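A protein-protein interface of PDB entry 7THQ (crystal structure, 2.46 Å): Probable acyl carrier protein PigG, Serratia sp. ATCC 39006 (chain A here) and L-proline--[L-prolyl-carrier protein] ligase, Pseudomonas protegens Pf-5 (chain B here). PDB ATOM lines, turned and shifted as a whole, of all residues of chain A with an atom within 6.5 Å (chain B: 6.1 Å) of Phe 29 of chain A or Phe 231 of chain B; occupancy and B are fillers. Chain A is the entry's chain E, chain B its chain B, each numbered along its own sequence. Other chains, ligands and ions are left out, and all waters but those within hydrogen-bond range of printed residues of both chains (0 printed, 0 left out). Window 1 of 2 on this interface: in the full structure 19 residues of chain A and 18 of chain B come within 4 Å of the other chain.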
ATOM      1  N   THR A  26      26.095   9.845 -24.060  1.00  0.00           N
ATOM      2  CA  THR A  26      25.646   8.905 -25.090  1.00  0.00           C
ATOM      3  C   THR A  26      24.304   8.270 -24.723  1.00  0.00           C
ATOM      4  O   THR A  26      24.126   7.825 -23.581  1.00  0.00           O
ATOM      5  CB  THR A  26      26.683   7.807 -25.320  1.00  0.00           C
ATOM      6  OG1 THR A  26      26.924   7.105 -24.094  1.00  0.00           O
ATOM      7  CG2 THR A  26      27.984   8.397 -25.844  1.00  0.00           C
ATOM      8  N   PRO A  27      23.341   8.211 -25.648  1.00  0.00           N
ATOM      9  CA  PRO A  27      22.037   7.598 -25.338  1.00  0.00           C
ATOM     10  C   PRO A  27      22.161   6.083 -25.262  1.00  0.00           C
ATOM     11  O   PRO A  27      22.494   5.426 -26.248  1.00  0.00           O
ATOM     12  CB  PRO A  27      21.155   8.022 -26.520  1.00  0.00           C
ATOM     13  CG  PRO A  27      21.882   9.154 -27.173  1.00  0.00           C
ATOM     14  CD  PRO A  27      23.335   8.851 -26.972  1.00  0.00           C
ATOM     15  N   LEU A  28      21.875   5.528 -24.082  1.00  0.00           N
ATOM     16  CA  LEU A  28      22.149   4.116 -23.842  1.00  0.00           C
ATOM     17  C   LEU A  28      21.087   3.203 -24.447  1.00  0.00           C
ATOM     18  O   LEU A  28      21.411   2.091 -24.880  1.00  0.00           O
ATOM     19  CB  LEU A  28      22.273   3.858 -22.341  1.00  0.00           C
ATOM     20  CG  LEU A  28      23.443   4.563 -21.652  1.00  0.00           C
ATOM     21  CD1 LEU A  28      23.581   4.084 -20.218  1.00  0.00           C
ATOM     22  CD2 LEU A  28      24.737   4.341 -22.427  1.00  0.00           C
ATOM     23  N   PHE A  29      19.827   3.638 -24.481  1.00  0.00           N
ATOM     24  CA  PHE A  29      18.752   2.806 -25.013  1.00  0.00           C
ATOM     25  C   PHE A  29      18.613   2.929 -26.524  1.00  0.00           C
ATOM     26  O   PHE A  29      18.360   1.927 -27.202  1.00  0.00           O
ATOM     27  CB  PHE A  29      17.430   3.150 -24.328  1.00  0.00           C
ATOM     28  CG  PHE A  29      17.372   2.702 -22.903  1.00  0.00           C
ATOM     29  CD1 PHE A  29      16.883   1.450 -22.577  1.00  0.00           C
ATOM     30  CD2 PHE A  29      17.836   3.524 -21.890  1.00  0.00           C
ATOM     31  CE1 PHE A  29      16.844   1.032 -21.264  1.00  0.00           C
ATOM     32  CE2 PHE A  29      17.799   3.112 -20.577  1.00  0.00           C
ATOM     33  CZ  PHE A  29      17.303   1.866 -20.264  1.00  0.00           C
ATOM     34  N   GLU A  30      18.769   4.140 -27.066  1.00  0.00           N
ATOM     35  CA  GLU A  30      18.715   4.314 -28.514  1.00  0.00           C
ATOM     36  C   GLU A  30      19.793   3.499 -29.215  1.00  0.00           C
ATOM     37  O   GLU A  30      19.621   3.105 -30.373  1.00  0.00           O
ATOM     38  CB  GLU A  30      18.873   5.789 -28.879  1.00  0.00           C
ATOM     39  CG  GLU A  30      17.904   6.732 -28.197  1.00  0.00           C
ATOM     40  CD  GLU A  30      18.049   8.152 -28.705  1.00  0.00           C
ATOM     41  OE1 GLU A  30      19.190   8.561 -29.007  1.00  0.00           O
ATOM     42  OE2 GLU A  30      17.027   8.862 -28.806  1.00  0.00           O
ATOM     43  N   LEU A  31      20.902   3.231 -28.529  1.00  0.00           N
ATOM     44  CA  LEU A  31      22.020   2.490 -29.092  1.00  0.00           C
ATOM     45  C   LEU A  31      22.033   1.029 -28.664  1.00  0.00           C
ATOM     46  O   LEU A  31      23.011   0.326 -28.938  1.00  0.00           O
ATOM     47  CB  LEU A  31      23.336   3.153 -28.685  1.00  0.00           C
ATOM     48  CG  LEU A  31      23.972   4.183 -29.617  1.00  0.00           C
ATOM     49  CD1 LEU A  31      22.973   5.265 -29.992  1.00  0.00           C
ATOM     50  CD2 LEU A  31      25.197   4.795 -28.955  1.00  0.00           C
ATOM     51  N   ASN A  32      20.970   0.557 -28.008  1.00  0.00           N
ATOM     52  CA  ASN A  32      20.875  -0.822 -27.515  1.00  0.00           C
ATOM     53  C   ASN A  32      22.118  -1.232 -26.725  1.00  0.00           C
ATOM     54  O   ASN A  32      22.490  -2.407 -26.688  1.00  0.00           O
ATOM     55  CB  ASN A  32      20.619  -1.800 -28.667  1.00  0.00           C
ATOM     56  CG  ASN A  32      20.056  -3.134 -28.196  1.00  0.00           C
ATOM     57  OD1 ASN A  32      19.338  -3.207 -27.198  1.00  0.00           O
ATOM     58  ND2 ASN A  32      20.386  -4.199 -28.918  1.00  0.00           N
ATOM     59  N   ILE A  33      22.777  -0.260 -26.089  1.00  0.00           N
ATOM     60  CA  ILE A  33      23.813  -0.590 -25.117  1.00  0.00           C
ATOM     61  C   ILE A  33      23.183  -1.249 -23.898  1.00  0.00           C
ATOM     62  O   ILE A  33      23.638  -2.297 -23.427  1.00  0.00           O
ATOM     63  CB  ILE A  33      24.610   0.666 -24.720  1.00  0.00           C
ATOM     64  CG1 ILE A  33      25.280   1.305 -25.936  1.00  0.00           C
ATOM     65  CG2 ILE A  33      25.643   0.317 -23.656  1.00  0.00           C
ATOM     66  CD1 ILE A  33      25.371   2.813 -25.837  1.00  0.00           C
ATOM     67  N   VAL A  34      22.116  -0.641 -23.385  1.00  0.00           N
ATOM     68  CA  VAL A  34      21.324  -1.157 -22.272  1.00  0.00           C
ATOM     69  C   VAL A  34      19.942  -1.505 -22.814  1.00  0.00           C
ATOM     70  O   VAL A  34      19.261  -0.644 -23.386  1.00  0.00           O
ATOM     71  CB  VAL A  34      21.219  -0.139 -21.129  1.00  0.00           C
ATOM     72  CG1 VAL A  34      20.304  -0.670 -20.044  1.00  0.00           C
ATOM     73  CG2 VAL A  34      22.598   0.185 -20.572  1.00  0.00           C
ATOM     74  N   ASP A  35      19.537  -2.764 -22.657  1.00  0.00           N
ATOM     75  CA  ASP A  35      18.241  -3.218 -23.127  1.00  0.00           C
ATOM     76  C   ASP A  35      17.159  -3.155 -22.045  1.00  0.00           C
ATOM     77  O   ASP A  35      17.334  -2.649 -20.940  1.00  0.00           O
ATOM     78  CB  ASP A  35      18.345  -4.640 -23.676  1.00  0.00           C
ATOM     79  N   SER A  36      16.013  -3.737 -22.384  1.00  0.00           N
ATOM     80  CA  SER A  36      14.863  -3.819 -21.485  1.00  0.00           C
ATOM     81  C   SER A  36      15.195  -4.590 -20.230  1.00  0.00           C
ATOM     82  O   SER A  36      14.851  -4.185 -19.107  1.00  0.00           O
ATOM     83  CB  SER A  36      13.763  -4.616 -22.155  1.00  0.00           C
ATOM     84  OG  SER A  36      13.656  -4.162 -23.472  1.00  0.00           O
ATOM     85  N   ILE A  39      17.950  -3.382 -17.338  1.00  0.00           N
ATOM     86  CA  ILE A  39      17.651  -2.120 -16.682  1.00  0.00           C
ATOM     87  C   ILE A  39      17.945  -2.200 -15.190  1.00  0.00           C
ATOM     88  O   ILE A  39      18.528  -1.274 -14.615  1.00  0.00           O
ATOM     89  CB  ILE A  39      16.186  -1.730 -16.963  1.00  0.00           C
ATOM     90  CG1 ILE A  39      15.907  -0.313 -16.477  1.00  0.00           C
ATOM     91  CG2 ILE A  39      15.203  -2.723 -16.335  1.00  0.00           C
ATOM     92  CD1 ILE A  39      16.772   0.713 -17.141  1.00  0.00           C
ATOM     93  N   PHE A  40      17.601  -3.319 -14.549  1.00  0.00           N
ATOM     94  CA  PHE A  40      17.832  -3.458 -13.116  1.00  0.00           C
ATOM     95  C   PHE A  40      19.270  -3.838 -12.797  1.00  0.00           C
ATOM     96  O   PHE A  40      19.756  -3.526 -11.704  1.00  0.00           O
ATOM     97  CB  PHE A  40      16.843  -4.447 -12.503  1.00  0.00           C
ATOM     98  CG  PHE A  40      15.516  -3.824 -12.181  1.00  0.00           C
ATOM     99  CD1 PHE A  40      15.319  -3.175 -10.972  1.00  0.00           C
ATOM    100  CD2 PHE A  40      14.475  -3.862 -13.093  1.00  0.00           C
ATOM    101  CE1 PHE A  40      14.104  -2.587 -10.673  1.00  0.00           C
ATOM    102  CE2 PHE A  40      13.256  -3.277 -12.800  1.00  0.00           C
ATOM    103  CZ  PHE A  40      13.071  -2.638 -11.588  1.00  0.00           C
ATOM    104  N   LEU A  42      21.584  -2.348 -13.947  1.00  0.00           N
ATOM    105  CA  LEU A  42      22.118  -1.006 -13.744  1.00  0.00           C
ATOM    106  C   LEU A  42      21.648  -0.408 -12.424  1.00  0.00           C
ATOM    107  O   LEU A  42      22.441   0.211 -11.704  1.00  0.00           O
ATOM    108  CB  LEU A  42      21.697  -0.091 -14.895  1.00  0.00           C
ATOM    109  CG  LEU A  42      22.641   0.078 -16.081  1.00  0.00           C
ATOM    110  CD1 LEU A  42      22.138   1.196 -16.981  1.00  0.00           C
ATOM    111  CD2 LEU A  42      24.050   0.366 -15.600  1.00  0.00           C
ATOM    112  N   GLU A  58      10.745   6.547  -9.660  1.00  0.00           N
ATOM    113  CA  GLU A  58      11.946   7.068 -10.291  1.00  0.00           C
ATOM    114  C   GLU A  58      12.632   6.042 -11.181  1.00  0.00           C
ATOM    115  O   GLU A  58      13.779   6.255 -11.585  1.00  0.00           O
ATOM    116  CB  GLU A  58      12.924   7.561  -9.221  1.00  0.00           C
ATOM    117  N   ILE A  59      11.936   4.968 -11.549  1.00  0.00           N
ATOM    118  CA  ILE A  59      12.441   4.060 -12.570  1.00  0.00           C
ATOM    119  C   ILE A  59      11.742   4.471 -13.860  1.00  0.00           C
ATOM    120  O   ILE A  59      10.954   3.716 -14.440  1.00  0.00           O
ATOM    121  CB  ILE A  59      12.207   2.577 -12.207  1.00  0.00           C
ATOM    122  CG1 ILE A  59      13.016   2.205 -10.966  1.00  0.00           C
ATOM    123  CG2 ILE A  59      12.678   1.648 -13.323  1.00  0.00           C
ATOM    124  CD1 ILE A  59      12.665   0.850 -10.386  1.00  0.00           C
ATOM    125  N   HIS A  60      11.949   5.721 -14.246  1.00  0.00           N
ATOM    126  CA  HIS A  60      11.554   6.446 -15.439  1.00  0.00           C
ATOM    127  C   HIS A  60      12.638   6.307 -16.506  1.00  0.00           C
ATOM    128  O   HIS A  60      13.829   6.244 -16.182  1.00  0.00           O
ATOM    129  CB  HIS A  60      11.326   7.920 -15.110  1.00  0.00           C
ATOM    130  CG  HIS A  60      10.607   8.681 -16.181  1.00  0.00           C
ATOM    131  ND1 HIS A  60       9.285   9.052 -16.070  1.00  0.00           N
ATOM    132  CD2 HIS A  60      11.033   9.160 -17.373  1.00  0.00           C
ATOM    133  CE1 HIS A  60       8.922   9.711 -17.157  1.00  0.00           C
ATOM    134  NE2 HIS A  60       9.965   9.790 -17.963  1.00  0.00           N
ATOM    135  N   PRO A  61      12.267   6.253 -17.789  1.00  0.00           N
ATOM    136  CA  PRO A  61      13.300   6.134 -18.831  1.00  0.00           C
ATOM    137  C   PRO A  61      14.207   7.348 -18.935  1.00  0.00           C
ATOM    138  O   PRO A  61      15.378   7.199 -19.307  1.00  0.00           O
ATOM    139  CB  PRO A  61      12.484   5.927 -20.116  1.00  0.00           C
ATOM    140  CG  PRO A  61      11.084   6.354 -19.770  1.00  0.00           C
ATOM    141  CD  PRO A  61      10.917   6.022 -18.325  1.00  0.00           C
ATOM    142  N   ALA A  62      13.705   8.544 -18.617  1.00  0.00           N
ATOM    143  CA  ALA A  62      14.534   9.745 -18.681  1.00  0.00           C
ATOM    144  C   ALA A  62      15.693   9.685 -17.694  1.00  0.00           C
ATOM    145  O   ALA A  62      16.774  10.209 -17.979  1.00  0.00           O
ATOM    146  CB  ALA A  62      13.683  10.990 -18.431  1.00  0.00           C
ATOM    147  N   PHE A  64      17.395   7.076 -16.801  1.00  0.00           N
ATOM    148  CA  PHE A  64      18.388   6.086 -17.190  1.00  0.00           C
ATOM    149  C   PHE A  64      18.804   6.205 -18.649  1.00  0.00           C
ATOM    150  O   PHE A  64      19.624   5.402 -19.111  1.00  0.00           O
ATOM    151  CB  PHE A  64      17.862   4.672 -16.913  1.00  0.00           C
ATOM    152  CG  PHE A  64      17.560   4.413 -15.464  1.00  0.00           C
ATOM    153  CD1 PHE A  64      18.449   3.703 -14.674  1.00  0.00           C
ATOM    154  CD2 PHE A  64      16.385   4.877 -14.892  1.00  0.00           C
ATOM    155  CE1 PHE A  64      18.177   3.464 -13.339  1.00  0.00           C
ATOM    156  CE2 PHE A  64      16.107   4.643 -13.558  1.00  0.00           C
ATOM    157  CZ  PHE A  64      17.005   3.933 -12.781  1.00  0.00           C
ATOM    158  N   ALA A  65      18.246   7.169 -19.386  1.00  0.00           N
ATOM    159  CA  ALA A  65      18.639   7.387 -20.776  1.00  0.00           C
ATOM    160  C   ALA A  65      20.152   7.515 -20.921  1.00  0.00           C
ATOM    161  O   ALA A  65      20.758   6.901 -21.807  1.00  0.00           O
ATOM    162  CB  ALA A  65      17.938   8.632 -21.322  1.00  0.00           C
ATOM    163  N   THR A  66      20.781   8.307 -20.055  1.00  0.00           N
ATOM    164  CA  THR A  66      22.207   8.575 -20.159  1.00  0.00           C
ATOM    165  C   THR A  66      22.849   8.502 -18.778  1.00  0.00           C
ATOM    166  O   THR A  66      22.168   8.474 -17.750  1.00  0.00           O
ATOM    167  CB  THR A  66      22.469   9.933 -20.829  1.00  0.00           C
ATOM    168  OG1 THR A  66      23.849  10.025 -21.207  1.00  0.00           O
ATOM    169  CG2 THR A  66      22.115  11.082 -19.908  1.00  0.00           C
ATOM    170  N   PRO B 226       1.026   3.720 -21.357  1.00  0.00           N
ATOM    171  CA  PRO B 226       2.064   4.642 -21.826  1.00  0.00           C
ATOM    172  C   PRO B 226       3.460   4.094 -21.578  1.00  0.00           C
ATOM    173  O   PRO B 226       3.701   3.349 -20.625  1.00  0.00           O
ATOM    174  CB  PRO B 226       1.817   5.908 -20.999  1.00  0.00           C
ATOM    175  CG  PRO B 226       1.121   5.438 -19.775  1.00  0.00           C
ATOM    176  CD  PRO B 226       0.395   4.167 -20.104  1.00  0.00           C
ATOM    177  N   GLU B 227       4.385   4.468 -22.467  1.00  0.00           N
ATOM    178  CA  GLU B 227       5.758   3.980 -22.361  1.00  0.00           C
ATOM    179  C   GLU B 227       6.388   4.328 -21.017  1.00  0.00           C
ATOM    180  O   GLU B 227       7.220   3.566 -20.509  1.00  0.00           O
ATOM    181  CB  GLU B 227       6.601   4.548 -23.504  1.00  0.00           C
ATOM    182  N   SER B 228       6.018   5.471 -20.429  1.00  0.00           N
ATOM    183  CA  SER B 228       6.559   5.847 -19.125  1.00  0.00           C
ATOM    184  C   SER B 228       6.150   4.859 -18.038  1.00  0.00           C
ATOM    185  O   SER B 228       6.898   4.651 -17.074  1.00  0.00           O
ATOM    186  CB  SER B 228       6.132   7.269 -18.759  1.00  0.00           C
ATOM    187  OG  SER B 228       4.723   7.395 -18.717  1.00  0.00           O
ATOM    188  N   ILE B 229       4.981   4.236 -18.174  1.00  0.00           N
ATOM    189  CA  ILE B 229       4.528   3.284 -17.166  1.00  0.00           C
ATOM    190  C   ILE B 229       4.960   1.870 -17.541  1.00  0.00           C
ATOM    191  O   ILE B 229       5.213   1.043 -16.658  1.00  0.00           O
ATOM    192  CB  ILE B 229       2.998   3.374 -17.002  1.00  0.00           C
ATOM    193  CG1 ILE B 229       2.587   4.752 -16.477  1.00  0.00           C
ATOM    194  CG2 ILE B 229       2.477   2.284 -16.076  1.00  0.00           C
ATOM    195  CD1 ILE B 229       2.693   4.899 -14.977  1.00  0.00           C
ATOM    196  N   ALA B 230       5.094   1.593 -18.841  1.00  0.00           N
ATOM    197  CA  ALA B 230       5.538   0.292 -19.322  1.00  0.00           C
ATOM    198  C   ALA B 230       6.950  -0.039 -18.860  1.00  0.00           C
ATOM    199  O   ALA B 230       7.370  -1.196 -18.975  1.00  0.00           O
ATOM    200  CB  ALA B 230       5.459   0.235 -20.848  1.00  0.00           C
ATOM    201  N   PHE B 231       7.685   0.945 -18.338  1.00  0.00           N
ATOM    202  CA  PHE B 231       9.119   0.837 -18.115  1.00  0.00           C
ATOM    203  C   PHE B 231       9.474   0.631 -16.650  1.00  0.00           C
ATOM    204  O   PHE B 231      10.589   0.189 -16.350  1.00  0.00           O
ATOM    205  CB  PHE B 231       9.779   2.124 -18.642  1.00  0.00           C
ATOM    206  CG  PHE B 231      11.252   2.236 -18.379  1.00  0.00           C
ATOM    207  CD1 PHE B 231      12.172   1.786 -19.306  1.00  0.00           C
ATOM    208  CD2 PHE B 231      11.716   2.855 -17.228  1.00  0.00           C
ATOM    209  CE1 PHE B 231      13.528   1.912 -19.071  1.00  0.00           C
ATOM    210  CE2 PHE B 231      13.065   2.982 -16.985  1.00  0.00           C
ATOM    211  CZ  PHE B 231      13.973   2.514 -17.908  1.00  0.00           C
ATOM    212  N   SER B 232       8.546   0.906 -15.742  1.00  0.00           N
ATOM    213  CA  SER B 232       8.659   0.483 -14.358  1.00  0.00           C
ATOM    214  C   SER B 232       7.756  -0.718 -14.144  1.00  0.00           C
ATOM    215  O   SER B 232       6.527  -0.550 -14.115  1.00  0.00           O
ATOM    216  CB  SER B 232       8.286   1.609 -13.401  1.00  0.00           C
ATOM    217  OG  SER B 232       8.765   1.343 -12.093  1.00  0.00           O
ATOM    218  N   PRO B 233       8.289  -1.934 -14.024  1.00  0.00           N
ATOM    219  CA  PRO B 233       7.403  -3.090 -13.824  1.00  0.00           C
ATOM    220  C   PRO B 233       6.510  -2.902 -12.615  1.00  0.00           C
ATOM    221  O   PRO B 233       5.367  -3.374 -12.612  1.00  0.00           O
ATOM    222  CB  PRO B 233       8.385  -4.254 -13.651  1.00  0.00           C
ATOM    223  CG  PRO B 233       9.572  -3.831 -14.459  1.00  0.00           C
ATOM    224  CD  PRO B 233       9.691  -2.347 -14.211  1.00  0.00           C
ATOM    225  N   LEU B 236       3.722  -0.866 -13.999  1.00  0.00           N
ATOM    226  CA  LEU B 236       2.839  -1.693 -14.818  1.00  0.00           C
ATOM    227  C   LEU B 236       1.819  -2.440 -13.968  1.00  0.00           C
ATOM    228  O   LEU B 236       0.624  -2.455 -14.279  1.00  0.00           O
ATOM    229  CB  LEU B 236       3.648  -2.695 -15.647  1.00  0.00           C
ATOM    230  CG  LEU B 236       3.926  -2.373 -17.114  1.00  0.00           C
ATOM    231  CD1 LEU B 236       4.753  -3.481 -17.755  1.00  0.00           C
ATOM    232  CD2 LEU B 236       2.612  -2.187 -17.860  1.00  0.00           C
ATOM    233  N   ARG B 466      15.768   0.005 -32.251  1.00  0.00           N
ATOM    234  CA  ARG B 466      16.803  -0.244 -31.249  1.00  0.00           C
ATOM    235  C   ARG B 466      16.969  -1.731 -30.953  1.00  0.00           C
ATOM    236  O   ARG B 466      18.096  -2.212 -30.781  1.00  0.00           O
ATOM    237  CB  ARG B 466      16.484   0.521 -29.965  1.00  0.00           C
ATOM    238  CG  ARG B 466      15.169   0.115 -29.330  1.00  0.00           C
ATOM    239  CD  ARG B 466      14.728   1.086 -28.262  1.00  0.00           C
ATOM    240  NE  ARG B 466      14.695   2.461 -28.743  1.00  0.00           N
ATOM    241  CZ  ARG B 466      14.452   3.510 -27.966  1.00  0.00           C
ATOM    242  NH1 ARG B 466      14.212   3.335 -26.673  1.00  0.00           N
ATOM    243  NH2 ARG B 466      14.439   4.732 -28.481  1.00  0.00           N
ATOM    244  N   ILE B 469      19.430  -3.539 -33.190  1.00  0.00           N
ATOM    245  CA  ILE B 469      20.854  -3.254 -33.132  1.00  0.00           C
ATOM    246  C   ILE B 469      21.555  -4.389 -32.397  1.00  0.00           C
ATOM    247  O   ILE B 469      21.037  -4.927 -31.409  1.00  0.00           O
ATOM    248  CB  ILE B 469      21.104  -1.899 -32.446  1.00  0.00           C
ATOM    249  CG1 ILE B 469      20.291  -0.794 -33.125  1.00  0.00           C
ATOM    250  CG2 ILE B 469      22.583  -1.550 -32.457  1.00  0.00           C
ATOM    251  CD1 ILE B 469      20.319   0.525 -32.382  1.00  0.00           C
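ND2 of Asn 32 of chain A lies within hydrogen-bond range of O of Ile 469 of chain B, 2.7 Å away.
Among the printed residues, pairs that only touch across the chains: Phe 29 of chain A with Phe 231 of chain B (3.96 Å), Phe 29 of chain A with Arg 466 of chain B (3.6 Å), Glu 30 of chain A with Ile 469 of chain B (3.3 Å), Asn 32 of chain A with Arg 466 of chain B (3.3 Å), Ile 39 of chain A with Phe 231 of chain B (3.4 Å), Phe 40 of chain A with Pro 233 of chain B (3.9 Å), Ile 59 of chain A with Phe 231 of chain B (3.0 Å), Ile 59 of chain A with Ser 232 of chain B (3.6 Å), His 60 of chain A with Phe 231 of chain B (3.4 Å) and Pro 61 of chain A with Phe 231 of chain B (3.4 Å).
Of the printed residues of chain B, Phe 29 of chain A touches Phe 231 (3.96 Å) and Arg 466 (3.6 Å). Printed residues of chain B within 4 Å of Glu 30 of chain A: Ile 469. Of the printed residues of chain B, Pro 61 of chain A touches Phe 231 (3.4 Å). Phe 231 of chain B touches just these residues of chain A: Phe 29, Ile 39, Ile 59, His 60 and Pro 61. Of the printed residues of chain A, Ser 232 of chain B touches Ile 59 (3.6 Å). Of the printed residues of chain A, Arg 466 of chain B touches Phe 29 and Asn 32. The nearest residue of chain A that does not touch Phe 231 of chain B is Phe 64 of chain A (4.4 Å). The nearest printed residue of chain B that does not touch Ile 59 of chain A is Ser 228 of chain B (4.9 Å).
Printed residues of chain A that touch a printed residue of chain B: Phe 29, Glu 30, Asn 32, Ile 39, Phe 40, Ile 59, His 60 and Pro 61. Hydrophobic or aromatic side chains of chain A within 4 Å of the printed part of chain B: Phe 29, Ile 39, Phe 40, Ile 59 and Pro 61. Of the 11 printed residues of chain B, 5 touch a printed residue of chain A. Hydrophobic or aromatic side chains of chain B within 4 Å of the printed part of chain A: Phe 231, Pro 233 and Ile 469. Among the printed residues, 11 pairs touch across the chains. Among the printed residues, no Asp or Glu carboxylate lies within 4 Å of a Lys or Arg side-chain nitrogen of the other chain.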
